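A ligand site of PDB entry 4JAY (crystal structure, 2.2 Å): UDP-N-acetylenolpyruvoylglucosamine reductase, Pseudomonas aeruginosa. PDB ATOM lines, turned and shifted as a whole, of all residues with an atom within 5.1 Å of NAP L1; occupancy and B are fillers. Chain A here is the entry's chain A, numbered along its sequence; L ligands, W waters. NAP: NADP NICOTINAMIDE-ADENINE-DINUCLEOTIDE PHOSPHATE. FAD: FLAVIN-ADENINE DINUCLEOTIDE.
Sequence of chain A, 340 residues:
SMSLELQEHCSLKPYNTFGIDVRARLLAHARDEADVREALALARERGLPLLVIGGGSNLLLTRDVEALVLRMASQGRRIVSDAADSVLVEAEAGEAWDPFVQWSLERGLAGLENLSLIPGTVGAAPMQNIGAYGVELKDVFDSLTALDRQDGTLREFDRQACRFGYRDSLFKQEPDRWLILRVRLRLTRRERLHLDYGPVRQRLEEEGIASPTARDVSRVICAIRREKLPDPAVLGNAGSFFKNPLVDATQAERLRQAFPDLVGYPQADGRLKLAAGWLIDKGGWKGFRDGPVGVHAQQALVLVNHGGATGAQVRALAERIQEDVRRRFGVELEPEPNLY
The backbone NH of Gly 131 is in hydrogen-bond range of an oxygen (O2) of FAD L2. O4 of FAD L2 sits at hydrogen-bond distance from NH1 of Arg 225, at 2.7 Å. A nitrogen (N7A) of NAP L1 sits close to the side-chain hydroxyl (OH) of Tyr 265, at 3.5 Å. An oxygen (O2N) of NAP L1 is in salt-bridge range of the side-chain amino group (NZ) of Lys 228. A nitrogen (N7N) of NAP L1 is in hydrogen-bond range of the side-chain carboxylate (OE2) of Glu 336, 2.9 Å away. An oxygen (O3D) of NAP L1 sits at hydrogen-bond distance from the backbone NH (N) of Tyr 133, at 3.0 Å. The guanidinium group (NH2) of Arg 167 sits at hydrogen-bond distance from an oxygen (O2D) of NAP L1, 3.0 Å away. The side-chain amide nitrogen of Gln 128 sits at hydrogen-bond distance from an oxygen (O2) of FAD L2. The backbone carbonyl oxygen (O) of Gly 131 lies within hydrogen-bond range of a nitrogen (N3) of FAD L2, at 2.9 Å. The side-chain amino group of Lys 273 lies within salt-bridge range of an oxygen (O2X) of NAP L1, 3.1 Å away. OH of Tyr 197 sits at hydrogen-bond distance from O3X of NAP L1. ND2 of Asn 244 is in hydrogen-bond range of O3B of NAP L1 (2.9 Å). O7N of NAP L1 is in hydrogen-bond range of N of Ser 240 (2.8 Å).
Water W3 bridges the side-chain amide nitrogen (ND2) of Asn 244 (3.0 Å) and an oxygen (O3B) of NAP L1 (3.0 Å). Water W1 lies within hydrogen-bond range of the backbone carbonyl oxygen (O) of Asp 196 (3.0 Å) and a nitrogen (N6A) of NAP L1 (3.1 Å). Water W4 lies within hydrogen-bond range of O3B of NAP L1 (3.1 Å) and OD1 of Asn 244 (3.1 Å).
Merely in contact with NAP L1: Ala 132 (3.4 Å), Asp 196 (3.7 Å), Gly 239 (3.7 Å), Gln 299 (3.7 Å), Tyr 166 (3.7 Å), Leu 229 (3.8 Å) and Arg 225 (3.9 Å). Hydrophobic or aromatic side chains within 4 Å of NAP L1: Ala 132, Tyr 133, Tyr 166, Tyr 197, Leu 229 and Tyr 265.
NH2 of Arg 167 is in hydrogen-bond range of O of Gly 131 (3.2 Å). The side-chain carboxylate of Glu 336 lies within hydrogen-bond range of the side-chain amide nitrogen of Gln 128, 2.8 Å away. ND2 of Asn 244 is in hydrogen-bond range of OH of Tyr 166, at 3.0 Å. N of Tyr 265 lies within hydrogen-bond range of O of Lys 273, at 2.7 Å. The side-chain carboxylate (OE1) of Glu 336 lies within salt-bridge range of the guanidinium group (NE) of Arg 167, 3.3 Å away.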
ATOM      1  N   GLN A 128      25.028 -26.334 -19.507  1.00  0.00           N
ATOM      2  CA  GLN A 128      25.309 -24.895 -19.674  1.00  0.00           C
ATOM      3  C   GLN A 128      24.090 -24.070 -19.899  1.00  0.00           C
ATOM      4  O   GLN A 128      24.193 -22.945 -20.354  1.00  0.00           O
ATOM      5  CB  GLN A 128      26.400 -24.597 -20.703  1.00  0.00           C
ATOM      6  CG  GLN A 128      26.051 -24.651 -22.208  1.00  0.00           C
ATOM      7  CD  GLN A 128      27.036 -23.863 -23.034  1.00  0.00           C
ATOM      8  OE1 GLN A 128      28.139 -23.546 -22.543  1.00  0.00           O
ATOM      9  NE2 GLN A 128      26.671 -23.521 -24.275  1.00  0.00           N
ATOM     10  N   GLY A 131      21.317 -21.782 -24.566  1.00  0.00           N
ATOM     11  CA  GLY A 131      20.552 -20.609 -24.962  1.00  0.00           C
ATOM     12  C   GLY A 131      20.960 -20.089 -26.312  1.00  0.00           C
ATOM     13  O   GLY A 131      22.123 -20.206 -26.701  1.00  0.00           O
ATOM     14  N   ALA A 132      20.016 -19.463 -26.970  1.00  0.00           N
ATOM     15  CA  ALA A 132      20.244 -18.774 -28.226  1.00  0.00           C
ATOM     16  C   ALA A 132      19.019 -17.879 -28.507  1.00  0.00           C
ATOM     17  O   ALA A 132      17.915 -18.219 -28.164  1.00  0.00           O
ATOM     18  CB  ALA A 132      20.409 -19.777 -29.359  1.00  0.00           C
ATOM     19  N   TYR A 133      19.235 -16.752 -29.151  1.00  0.00           N
ATOM     20  CA  TYR A 133      18.180 -15.895 -29.558  1.00  0.00           C
ATOM     21  C   TYR A 133      17.263 -15.487 -28.408  1.00  0.00           C
ATOM     22  O   TYR A 133      16.056 -15.403 -28.578  1.00  0.00           O
ATOM     23  CB  TYR A 133      17.473 -16.531 -30.786  1.00  0.00           C
ATOM     24  CG  TYR A 133      18.455 -16.614 -31.935  1.00  0.00           C
ATOM     25  CD1 TYR A 133      18.948 -15.466 -32.561  1.00  0.00           C
ATOM     26  CD2 TYR A 133      18.968 -17.823 -32.354  1.00  0.00           C
ATOM     27  CE1 TYR A 133      19.881 -15.543 -33.577  1.00  0.00           C
ATOM     28  CE2 TYR A 133      19.905 -17.892 -33.385  1.00  0.00           C
ATOM     29  CZ  TYR A 133      20.349 -16.745 -33.995  1.00  0.00           C
ATOM     30  OH  TYR A 133      21.321 -16.828 -34.999  1.00  0.00           O
ATOM     31  N   GLY A 134      17.849 -15.189 -27.247  1.00  0.00           N
ATOM     32  CA  GLY A 134      17.114 -14.665 -26.094  1.00  0.00           C
ATOM     33  C   GLY A 134      16.341 -15.679 -25.287  1.00  0.00           C
ATOM     34  O   GLY A 134      15.549 -15.331 -24.419  1.00  0.00           O
ATOM     35  N   TYR A 166      23.652 -17.653 -16.589  1.00  0.00           N
ATOM     36  CA  TYR A 166      24.117 -17.456 -17.965  1.00  0.00           C
ATOM     37  C   TYR A 166      25.286 -18.450 -18.228  1.00  0.00           C
ATOM     38  O   TYR A 166      26.338 -18.362 -17.586  1.00  0.00           O
ATOM     39  CB  TYR A 166      24.493 -15.969 -18.199  1.00  0.00           C
ATOM     40  CG  TYR A 166      25.127 -15.786 -19.513  1.00  0.00           C
ATOM     41  CD1 TYR A 166      24.389 -15.946 -20.698  1.00  0.00           C
ATOM     42  CD2 TYR A 166      26.468 -15.551 -19.593  1.00  0.00           C
ATOM     43  CE1 TYR A 166      24.993 -15.831 -21.934  1.00  0.00           C
ATOM     44  CE2 TYR A 166      27.099 -15.447 -20.823  1.00  0.00           C
ATOM     45  CZ  TYR A 166      26.363 -15.591 -21.992  1.00  0.00           C
ATOM     46  OH  TYR A 166      27.032 -15.480 -23.203  1.00  0.00           O
ATOM     47  N   ARG A 167      25.053 -19.389 -19.131  1.00  0.00           N
ATOM     48  CA  ARG A 167      25.982 -20.508 -19.442  1.00  0.00           C
ATOM     49  C   ARG A 167      26.445 -21.264 -18.174  1.00  0.00           C
ATOM     50  O   ARG A 167      27.609 -21.656 -18.050  1.00  0.00           O
ATOM     51  CB  ARG A 167      27.165 -20.056 -20.277  1.00  0.00           C
ATOM     52  CG  ARG A 167      26.806 -19.459 -21.631  1.00  0.00           C
ATOM     53  CD  ARG A 167      26.066 -20.437 -22.532  1.00  0.00           C
ATOM     54  NE  ARG A 167      25.915 -19.984 -23.920  1.00  0.00           N
ATOM     55  CZ  ARG A 167      24.896 -19.281 -24.384  1.00  0.00           C
ATOM     56  NH1 ARG A 167      23.909 -18.905 -23.577  1.00  0.00           N
ATOM     57  NH2 ARG A 167      24.843 -18.932 -25.668  1.00  0.00           N
ATOM     58  N   ASP A 196      12.976 -11.331 -29.664  1.00  0.00           N
ATOM     59  CA  ASP A 196      13.865 -10.332 -29.103  1.00  0.00           C
ATOM     60  C   ASP A 196      14.982  -9.911 -30.017  1.00  0.00           C
ATOM     61  O   ASP A 196      15.363  -8.772 -30.000  1.00  0.00           O
ATOM     62  CB  ASP A 196      14.530 -10.856 -27.823  1.00  0.00           C
ATOM     63  CG  ASP A 196      13.542 -11.340 -26.815  1.00  0.00           C
ATOM     64  OD1 ASP A 196      13.726 -11.007 -25.621  1.00  0.00           O
ATOM     65  OD2 ASP A 196      12.591 -12.050 -27.216  1.00  0.00           O
ATOM     66  N   TYR A 197      15.609 -10.828 -30.726  1.00  0.00           N
ATOM     67  CA  TYR A 197      16.832 -10.494 -31.477  1.00  0.00           C
ATOM     68  C   TYR A 197      16.389  -9.999 -32.825  1.00  0.00           C
ATOM     69  O   TYR A 197      15.667 -10.701 -33.508  1.00  0.00           O
ATOM     70  CB  TYR A 197      17.779 -11.721 -31.636  1.00  0.00           C
ATOM     71  CG  TYR A 197      18.590 -12.055 -30.400  1.00  0.00           C
ATOM     72  CD1 TYR A 197      18.039 -11.898 -29.142  1.00  0.00           C
ATOM     73  CD2 TYR A 197      19.879 -12.546 -30.499  1.00  0.00           C
ATOM     74  CE1 TYR A 197      18.738 -12.197 -28.006  1.00  0.00           C
ATOM     75  CE2 TYR A 197      20.595 -12.870 -29.359  1.00  0.00           C
ATOM     76  CZ  TYR A 197      20.014 -12.693 -28.110  1.00  0.00           C
ATOM     77  OH  TYR A 197      20.660 -12.965 -26.923  1.00  0.00           O
ATOM     78  N   GLY A 198      16.836  -8.792 -33.193  1.00  0.00           N
ATOM     79  CA  GLY A 198      16.421  -8.128 -34.421  1.00  0.00           C
ATOM     80  C   GLY A 198      16.472  -8.946 -35.705  1.00  0.00           C
ATOM     81  O   GLY A 198      15.519  -8.913 -36.473  1.00  0.00           O
ATOM     82  N   ARG A 225      21.093 -19.559 -38.705  1.00  0.00           N
ATOM     83  CA  ARG A 225      22.160 -20.385 -38.192  1.00  0.00           C
ATOM     84  C   ARG A 225      22.909 -21.108 -39.291  1.00  0.00           C
ATOM     85  O   ARG A 225      24.131 -21.246 -39.228  1.00  0.00           O
ATOM     86  CB  ARG A 225      21.598 -21.371 -37.161  1.00  0.00           C
ATOM     87  CG  ARG A 225      21.268 -20.702 -35.839  1.00  0.00           C
ATOM     88  CD  ARG A 225      20.825 -21.684 -34.780  1.00  0.00           C
ATOM     89  NE  ARG A 225      21.959 -22.485 -34.251  1.00  0.00           N
ATOM     90  CZ  ARG A 225      22.456 -22.383 -33.017  1.00  0.00           C
ATOM     91  NH1 ARG A 225      22.011 -21.497 -32.111  1.00  0.00           N
ATOM     92  NH2 ARG A 225      23.482 -23.144 -32.711  1.00  0.00           N
ATOM     93  N   LYS A 228      25.236 -18.648 -41.093  1.00  0.00           N
ATOM     94  CA  LYS A 228      26.373 -17.973 -40.517  1.00  0.00           C
ATOM     95  C   LYS A 228      27.337 -18.809 -39.682  1.00  0.00           C
ATOM     96  O   LYS A 228      28.507 -18.511 -39.623  1.00  0.00           O
ATOM     97  CB  LYS A 228      25.940 -16.673 -39.835  1.00  0.00           C
ATOM     98  CG  LYS A 228      25.337 -16.823 -38.476  1.00  0.00           C
ATOM     99  CD  LYS A 228      24.737 -15.481 -38.056  1.00  0.00           C
ATOM    100  CE  LYS A 228      25.797 -14.418 -37.866  1.00  0.00           C
ATOM    101  NZ  LYS A 228      25.344 -13.297 -37.006  1.00  0.00           N
ATOM    102  N   LEU A 229      26.869 -19.907 -39.103  1.00  0.00           N
ATOM    103  CA  LEU A 229      27.731 -20.780 -38.324  1.00  0.00           C
ATOM    104  C   LEU A 229      28.407 -21.827 -39.189  1.00  0.00           C
ATOM    105  O   LEU A 229      27.766 -22.463 -40.018  1.00  0.00           O
ATOM    106  CB  LEU A 229      26.947 -21.505 -37.250  1.00  0.00           C
ATOM    107  CG  LEU A 229      26.046 -20.612 -36.439  1.00  0.00           C
ATOM    108  CD1 LEU A 229      25.270 -21.489 -35.470  1.00  0.00           C
ATOM    109  CD2 LEU A 229      26.874 -19.545 -35.740  1.00  0.00           C
ATOM    110  N   ALA A 238      33.474 -26.129 -31.743  1.00  0.00           N
ATOM    111  CA  ALA A 238      32.541 -26.348 -30.657  1.00  0.00           C
ATOM    112  C   ALA A 238      31.730 -25.076 -30.457  1.00  0.00           C
ATOM    113  O   ALA A 238      31.427 -24.708 -29.336  1.00  0.00           O
ATOM    114  CB  ALA A 238      33.272 -26.686 -29.374  1.00  0.00           C
ATOM    115  N   GLY A 239      31.347 -24.450 -31.571  1.00  0.00           N
ATOM    116  CA  GLY A 239      30.624 -23.197 -31.523  1.00  0.00           C
ATOM    117  C   GLY A 239      31.397 -22.083 -30.823  1.00  0.00           C
ATOM    118  O   GLY A 239      32.606 -21.960 -31.001  1.00  0.00           O
ATOM    119  N   SER A 240      30.691 -21.238 -30.076  1.00  0.00           N
ATOM    120  CA  SER A 240      31.301 -20.171 -29.344  1.00  0.00           C
ATOM    121  C   SER A 240      32.265 -20.707 -28.348  1.00  0.00           C
ATOM    122  O   SER A 240      31.889 -21.494 -27.509  1.00  0.00           O
ATOM    123  CB  SER A 240      30.258 -19.324 -28.617  1.00  0.00           C
ATOM    124  OG  SER A 240      29.400 -18.734 -29.586  1.00  0.00           O
ATOM    125  N   ASN A 244      30.402 -14.695 -23.066  1.00  0.00           N
ATOM    126  CA  ASN A 244      30.310 -13.248 -23.002  1.00  0.00           C
ATOM    127  C   ASN A 244      30.477 -12.787 -21.572  1.00  0.00           C
ATOM    128  O   ASN A 244      29.712 -13.183 -20.729  1.00  0.00           O
ATOM    129  CB  ASN A 244      28.980 -12.787 -23.540  1.00  0.00           C
ATOM    130  CG  ASN A 244      28.842 -13.090 -25.023  1.00  0.00           C
ATOM    131  OD1 ASN A 244      29.744 -12.845 -25.833  1.00  0.00           O
ATOM    132  ND2 ASN A 244      27.691 -13.611 -25.396  1.00  0.00           N
ATOM    133  N   TYR A 265      25.344  -5.180 -23.583  1.00  0.00           N
ATOM    134  CA  TYR A 265      23.935  -5.202 -23.291  1.00  0.00           C
ATOM    135  C   TYR A 265      23.747  -5.095 -21.806  1.00  0.00           C
ATOM    136  O   TYR A 265      24.189  -5.979 -21.071  1.00  0.00           O
ATOM    137  CB  TYR A 265      23.366  -6.476 -23.821  1.00  0.00           C
ATOM    138  CG  TYR A 265      23.486  -6.547 -25.286  1.00  0.00           C
ATOM    139  CD1 TYR A 265      24.616  -7.108 -25.896  1.00  0.00           C
ATOM    140  CD2 TYR A 265      22.494  -6.061 -26.101  1.00  0.00           C
ATOM    141  CE1 TYR A 265      24.725  -7.201 -27.263  1.00  0.00           C
ATOM    142  CE2 TYR A 265      22.588  -6.138 -27.468  1.00  0.00           C
ATOM    143  CZ  TYR A 265      23.699  -6.709 -28.047  1.00  0.00           C
ATOM    144  OH  TYR A 265      23.759  -6.762 -29.402  1.00  0.00           O
ATOM    145  N   LYS A 273      26.733  -6.905 -20.156  1.00  0.00           N
ATOM    146  CA  LYS A 273      27.190  -8.059 -20.940  1.00  0.00           C
ATOM    147  C   LYS A 273      27.872  -7.586 -22.236  1.00  0.00           C
ATOM    148  O   LYS A 273      27.236  -7.040 -23.114  1.00  0.00           O
ATOM    149  CB  LYS A 273      26.024  -8.963 -21.307  1.00  0.00           C
ATOM    150  CG  LYS A 273      26.393 -10.301 -21.923  1.00  0.00           C
ATOM    151  CD  LYS A 273      25.146 -11.085 -22.396  1.00  0.00           C
ATOM    152  CE  LYS A 273      24.808 -10.781 -23.875  1.00  0.00           C
ATOM    153  NZ  LYS A 273      23.375 -10.919 -24.284  1.00  0.00           N
ATOM    154  N   ALA A 275      29.805  -8.114 -25.833  1.00  0.00           N
ATOM    155  CA  ALA A 275      29.959  -9.079 -26.887  1.00  0.00           C
ATOM    156  C   ALA A 275      31.428  -9.494 -26.925  1.00  0.00           C
ATOM    157  O   ALA A 275      32.296  -8.730 -27.332  1.00  0.00           O
ATOM    158  CB  ALA A 275      29.542  -8.511 -28.236  1.00  0.00           C
ATOM    159  N   GLN A 299      32.649 -15.223 -37.583  1.00  0.00           N
ATOM    160  CA  GLN A 299      32.276 -15.523 -36.177  1.00  0.00           C
ATOM    161  C   GLN A 299      33.502 -15.528 -35.226  1.00  0.00           C
ATOM    162  O   GLN A 299      34.173 -16.531 -35.025  1.00  0.00           O
ATOM    163  CB  GLN A 299      31.515 -16.828 -36.087  1.00  0.00           C
ATOM    164  CG  GLN A 299      30.341 -16.933 -37.027  1.00  0.00           C
ATOM    165  CD  GLN A 299      29.367 -15.780 -36.868  1.00  0.00           C
ATOM    166  OE1 GLN A 299      28.687 -15.649 -35.848  1.00  0.00           O
ATOM    167  NE2 GLN A 299      29.257 -14.961 -37.923  1.00  0.00           N
ATOM    168  N   GLU A 336      33.909 -21.573 -22.875  1.00  0.00           N
ATOM    169  CA  GLU A 336      32.658 -22.243 -22.747  1.00  0.00           C
ATOM    170  C   GLU A 336      32.828 -23.756 -22.879  1.00  0.00           C
ATOM    171  O   GLU A 336      32.265 -24.482 -22.115  1.00  0.00           O
ATOM    172  CB  GLU A 336      31.725 -21.711 -23.806  1.00  0.00           C
ATOM    173  CG  GLU A 336      30.314 -22.167 -23.648  1.00  0.00           C
ATOM    174  CD  GLU A 336      29.411 -21.621 -24.732  1.00  0.00           C
ATOM    175  OE1 GLU A 336      29.134 -20.395 -24.743  1.00  0.00           O
ATOM    176  OE2 GLU A 336      28.949 -22.428 -25.577  1.00  0.00           O
HETATM  177  PA  NAP L   1      24.485 -12.414 -32.768  1.00  0.00           P
HETATM  178  O1A NAP L   1      23.086 -12.925 -32.981  1.00  0.00           O
HETATM  179  O2A NAP L   1      25.222 -11.903 -33.984  1.00  0.00           O
HETATM  180  O5B NAP L   1      24.616 -11.480 -31.481  1.00  0.00           O
HETATM  181  C5B NAP L   1      25.957 -11.133 -31.149  1.00  0.00           C
HETATM  182  C4B NAP L   1      26.155 -10.958 -29.651  1.00  0.00           C
HETATM  183  O4B NAP L   1      25.286  -9.955 -29.141  1.00  0.00           O
HETATM  184  C3B NAP L   1      25.854 -12.166 -28.821  1.00  0.00           C
HETATM  185  O3B NAP L   1      26.842 -12.160 -27.768  1.00  0.00           O
HETATM  186  C2B NAP L   1      24.488 -11.985 -28.205  1.00  0.00           C
HETATM  187  O2B NAP L   1      24.490 -12.571 -26.889  1.00  0.00           O
HETATM  188  C1B NAP L   1      24.352 -10.474 -28.215  1.00  0.00           C
HETATM  189  N9A NAP L   1      23.027  -9.934 -28.662  1.00  0.00           N
HETATM  190  C8A NAP L   1      22.590  -9.712 -29.939  1.00  0.00           C
HETATM  191  N7A NAP L   1      21.331  -9.224 -29.935  1.00  0.00           N
HETATM  192  C5A NAP L   1      20.982  -9.121 -28.643  1.00  0.00           C
HETATM  193  C6A NAP L   1      19.785  -8.683 -27.915  1.00  0.00           C
HETATM  194  N6A NAP L   1      18.713  -8.254 -28.630  1.00  0.00           N
HETATM  195  N1A NAP L   1      19.814  -8.761 -26.553  1.00  0.00           N
HETATM  196  C2A NAP L   1      20.890  -9.181 -25.852  1.00  0.00           C
HETATM  197  N3A NAP L   1      22.008  -9.575 -26.473  1.00  0.00           N
HETATM  198  C4A NAP L   1      22.085  -9.587 -27.814  1.00  0.00           C
HETATM  199  O3  NAP L   1      25.385 -13.615 -32.183  1.00  0.00           O
HETATM  200  PN  NAP L   1      25.633 -14.982 -33.017  1.00  0.00           P
HETATM  201  O1N NAP L   1      27.023 -15.324 -32.560  1.00  0.00           O
HETATM  202  O2N NAP L   1      25.123 -14.715 -34.453  1.00  0.00           O
HETATM  203  O5D NAP L   1      24.677 -16.035 -32.251  1.00  0.00           O
HETATM  204  C5D NAP L   1      23.260 -16.049 -32.400  1.00  0.00           C
HETATM  205  C4D NAP L   1      22.669 -16.565 -31.095  1.00  0.00           C
HETATM  206  O4D NAP L   1      23.104 -17.910 -31.034  1.00  0.00           O
HETATM  207  C3D NAP L   1      23.206 -15.950 -29.808  1.00  0.00           C
HETATM  208  O3D NAP L   1      22.163 -15.971 -28.824  1.00  0.00           O
HETATM  209  C2D NAP L   1      24.365 -16.851 -29.417  1.00  0.00           C
HETATM  210  O2D NAP L   1      24.545 -17.030 -28.011  1.00  0.00           O
HETATM  211  C1D NAP L   1      23.945 -18.177 -29.963  1.00  0.00           C
HETATM  212  N1N NAP L   1      25.030 -19.041 -30.422  1.00  0.00           N
HETATM  213  C2N NAP L   1      25.698 -19.661 -29.451  1.00  0.00           C
HETATM  214  C3N NAP L   1      26.740 -20.531 -29.740  1.00  0.00           C
HETATM  215  C7N NAP L   1      27.436 -21.239 -28.637  1.00  0.00           C
HETATM  216  O7N NAP L   1      28.254 -22.080 -28.945  1.00  0.00           O
HETATM  217  N7N NAP L   1      27.155 -20.965 -27.403  1.00  0.00           N
HETATM  218  C4N NAP L   1      27.062 -20.815 -31.072  1.00  0.00           C
HETATM  219  C5N NAP L   1      26.340 -20.155 -32.073  1.00  0.00           C
HETATM  220  C6N NAP L   1      25.326 -19.249 -31.717  1.00  0.00           C
HETATM  221  P2B NAP L   1      24.079 -14.096 -26.455  1.00  0.00           P
HETATM  222  O1X NAP L   1      25.092 -15.000 -27.153  1.00  0.00           O
HETATM  223  O2X NAP L   1      24.175 -13.802 -24.946  1.00  0.00           O
HETATM  224  O3X NAP L   1      22.726 -14.422 -26.945  1.00  0.00           O
HETATM  225  PA  FAD L   2      29.076 -32.622 -24.794  1.00  0.00           P
HETATM  226  O1A FAD L   2      29.904 -31.702 -25.575  1.00  0.00           O
HETATM  227  O2A FAD L   2      29.099 -34.078 -25.155  1.00  0.00           O
HETATM  228  O5B FAD L   2      29.570 -32.394 -23.261  1.00  0.00           O
HETATM  229  C5B FAD L   2      29.150 -31.197 -22.581  1.00  0.00           C
HETATM  230  C4B FAD L   2      29.537 -31.190 -21.093  1.00  0.00           C
HETATM  231  O4B FAD L   2      28.486 -31.869 -20.395  1.00  0.00           O
HETATM  232  C3B FAD L   2      30.727 -32.079 -20.870  1.00  0.00           C
HETATM  233  O3B FAD L   2      31.375 -31.703 -19.699  1.00  0.00           O
HETATM  234  C2B FAD L   2      30.158 -33.467 -20.589  1.00  0.00           C
HETATM  235  O2B FAD L   2      31.035 -34.140 -19.763  1.00  0.00           O
HETATM  236  C1B FAD L   2      28.924 -33.168 -19.845  1.00  0.00           C
HETATM  237  N9A FAD L   2      27.808 -34.047 -20.093  1.00  0.00           N
HETATM  238  C8A FAD L   2      27.307 -34.317 -21.301  1.00  0.00           C
HETATM  239  N7A FAD L   2      26.230 -35.125 -21.178  1.00  0.00           N
HETATM  240  C5A FAD L   2      25.999 -35.285 -19.886  1.00  0.00           C
HETATM  241  C6A FAD L   2      25.005 -35.993 -19.118  1.00  0.00           C
HETATM  242  N6A FAD L   2      23.998 -36.699 -19.690  1.00  0.00           N
HETATM  243  N1A FAD L   2      25.108 -35.923 -17.786  1.00  0.00           N
HETATM  244  C2A FAD L   2      26.128 -35.260 -17.180  1.00  0.00           C
HETATM  245  N3A FAD L   2      27.086 -34.565 -17.822  1.00  0.00           N
HETATM  246  C4A FAD L   2      27.049 -34.574 -19.174  1.00  0.00           C
HETATM  247  N1  FAD L   2      25.351 -24.080 -27.128  1.00  0.00           N
HETATM  248  C2  FAD L   2      24.417 -23.152 -26.748  1.00  0.00           C
HETATM  249  O2  FAD L   2      24.092 -23.063 -25.546  1.00  0.00           O
HETATM  250  N3  FAD L   2      23.778 -22.375 -27.606  1.00  0.00           N
HETATM  251  C4  FAD L   2      23.996 -22.387 -28.924  1.00  0.00           C
HETATM  252  O4  FAD L   2      23.341 -21.617 -29.741  1.00  0.00           O
HETATM  253  C4X FAD L   2      24.992 -23.335 -29.381  1.00  0.00           C
HETATM  254  N5  FAD L   2      25.349 -23.399 -30.656  1.00  0.00           N
HETATM  255  C5X FAD L   2      26.286 -24.284 -31.085  1.00  0.00           C
HETATM  256  C6  FAD L   2      26.609 -24.353 -32.425  1.00  0.00           C
HETATM  257  C7  FAD L   2      27.552 -25.252 -32.873  1.00  0.00           C
HETATM  258  C7M FAD L   2      27.923 -25.362 -34.312  1.00  0.00           C
HETATM  259  C8  FAD L   2      28.234 -26.138 -31.945  1.00  0.00           C
HETATM  260  C8M FAD L   2      29.251 -27.121 -32.485  1.00  0.00           C
HETATM  261  C9  FAD L   2      27.944 -26.026 -30.608  1.00  0.00           C
HETATM  262  C9A FAD L   2      26.995 -25.169 -30.144  1.00  0.00           C
HETATM  263  N10 FAD L   2      26.647 -25.090 -28.778  1.00  0.00           N
HETATM  264  C10 FAD L   2      25.666 -24.189 -28.397  1.00  0.00           C
HETATM  265  C1' FAD L   2      27.274 -25.875 -27.759  1.00  0.00           C
HETATM  266  C2' FAD L   2      26.693 -27.247 -27.613  1.00  0.00           C
HETATM  267  O2' FAD L   2      26.076 -27.602 -28.833  1.00  0.00           O
HETATM  268  C3' FAD L   2      25.720 -27.274 -26.482  1.00  0.00           C
HETATM  269  O3' FAD L   2      26.313 -26.703 -25.275  1.00  0.00           O
HETATM  270  C4' FAD L   2      25.256 -28.723 -26.279  1.00  0.00           C
HETATM  271  O4' FAD L   2      24.338 -28.791 -25.173  1.00  0.00           O
HETATM  272  C5' FAD L   2      26.370 -29.682 -25.843  1.00  0.00           C
HETATM  273  O5' FAD L   2      25.781 -30.964 -25.891  1.00  0.00           O
HETATM  274  P   FAD L   2      26.616 -32.297 -26.066  1.00  0.00           P
HETATM  275  O1P FAD L   2      25.592 -33.362 -25.738  1.00  0.00           O
HETATM  276  O2P FAD L   2      27.383 -32.255 -27.294  1.00  0.00           O
HETATM  277  O3P FAD L   2      27.575 -32.157 -24.776  1.00  0.00           O
HETATM  278  O   HOH W   1      16.240  -6.469 -28.346  1.00  0.00           O
HETATM  279  O   HOH W   2      20.070 -12.157 -24.679  1.00  0.00           O
HETATM  280  O   HOH W   3      28.084 -14.907 -28.082  1.00  0.00           O
HETATM  281  O   HOH W   4      29.703 -12.253 -28.923  1.00  0.00           O
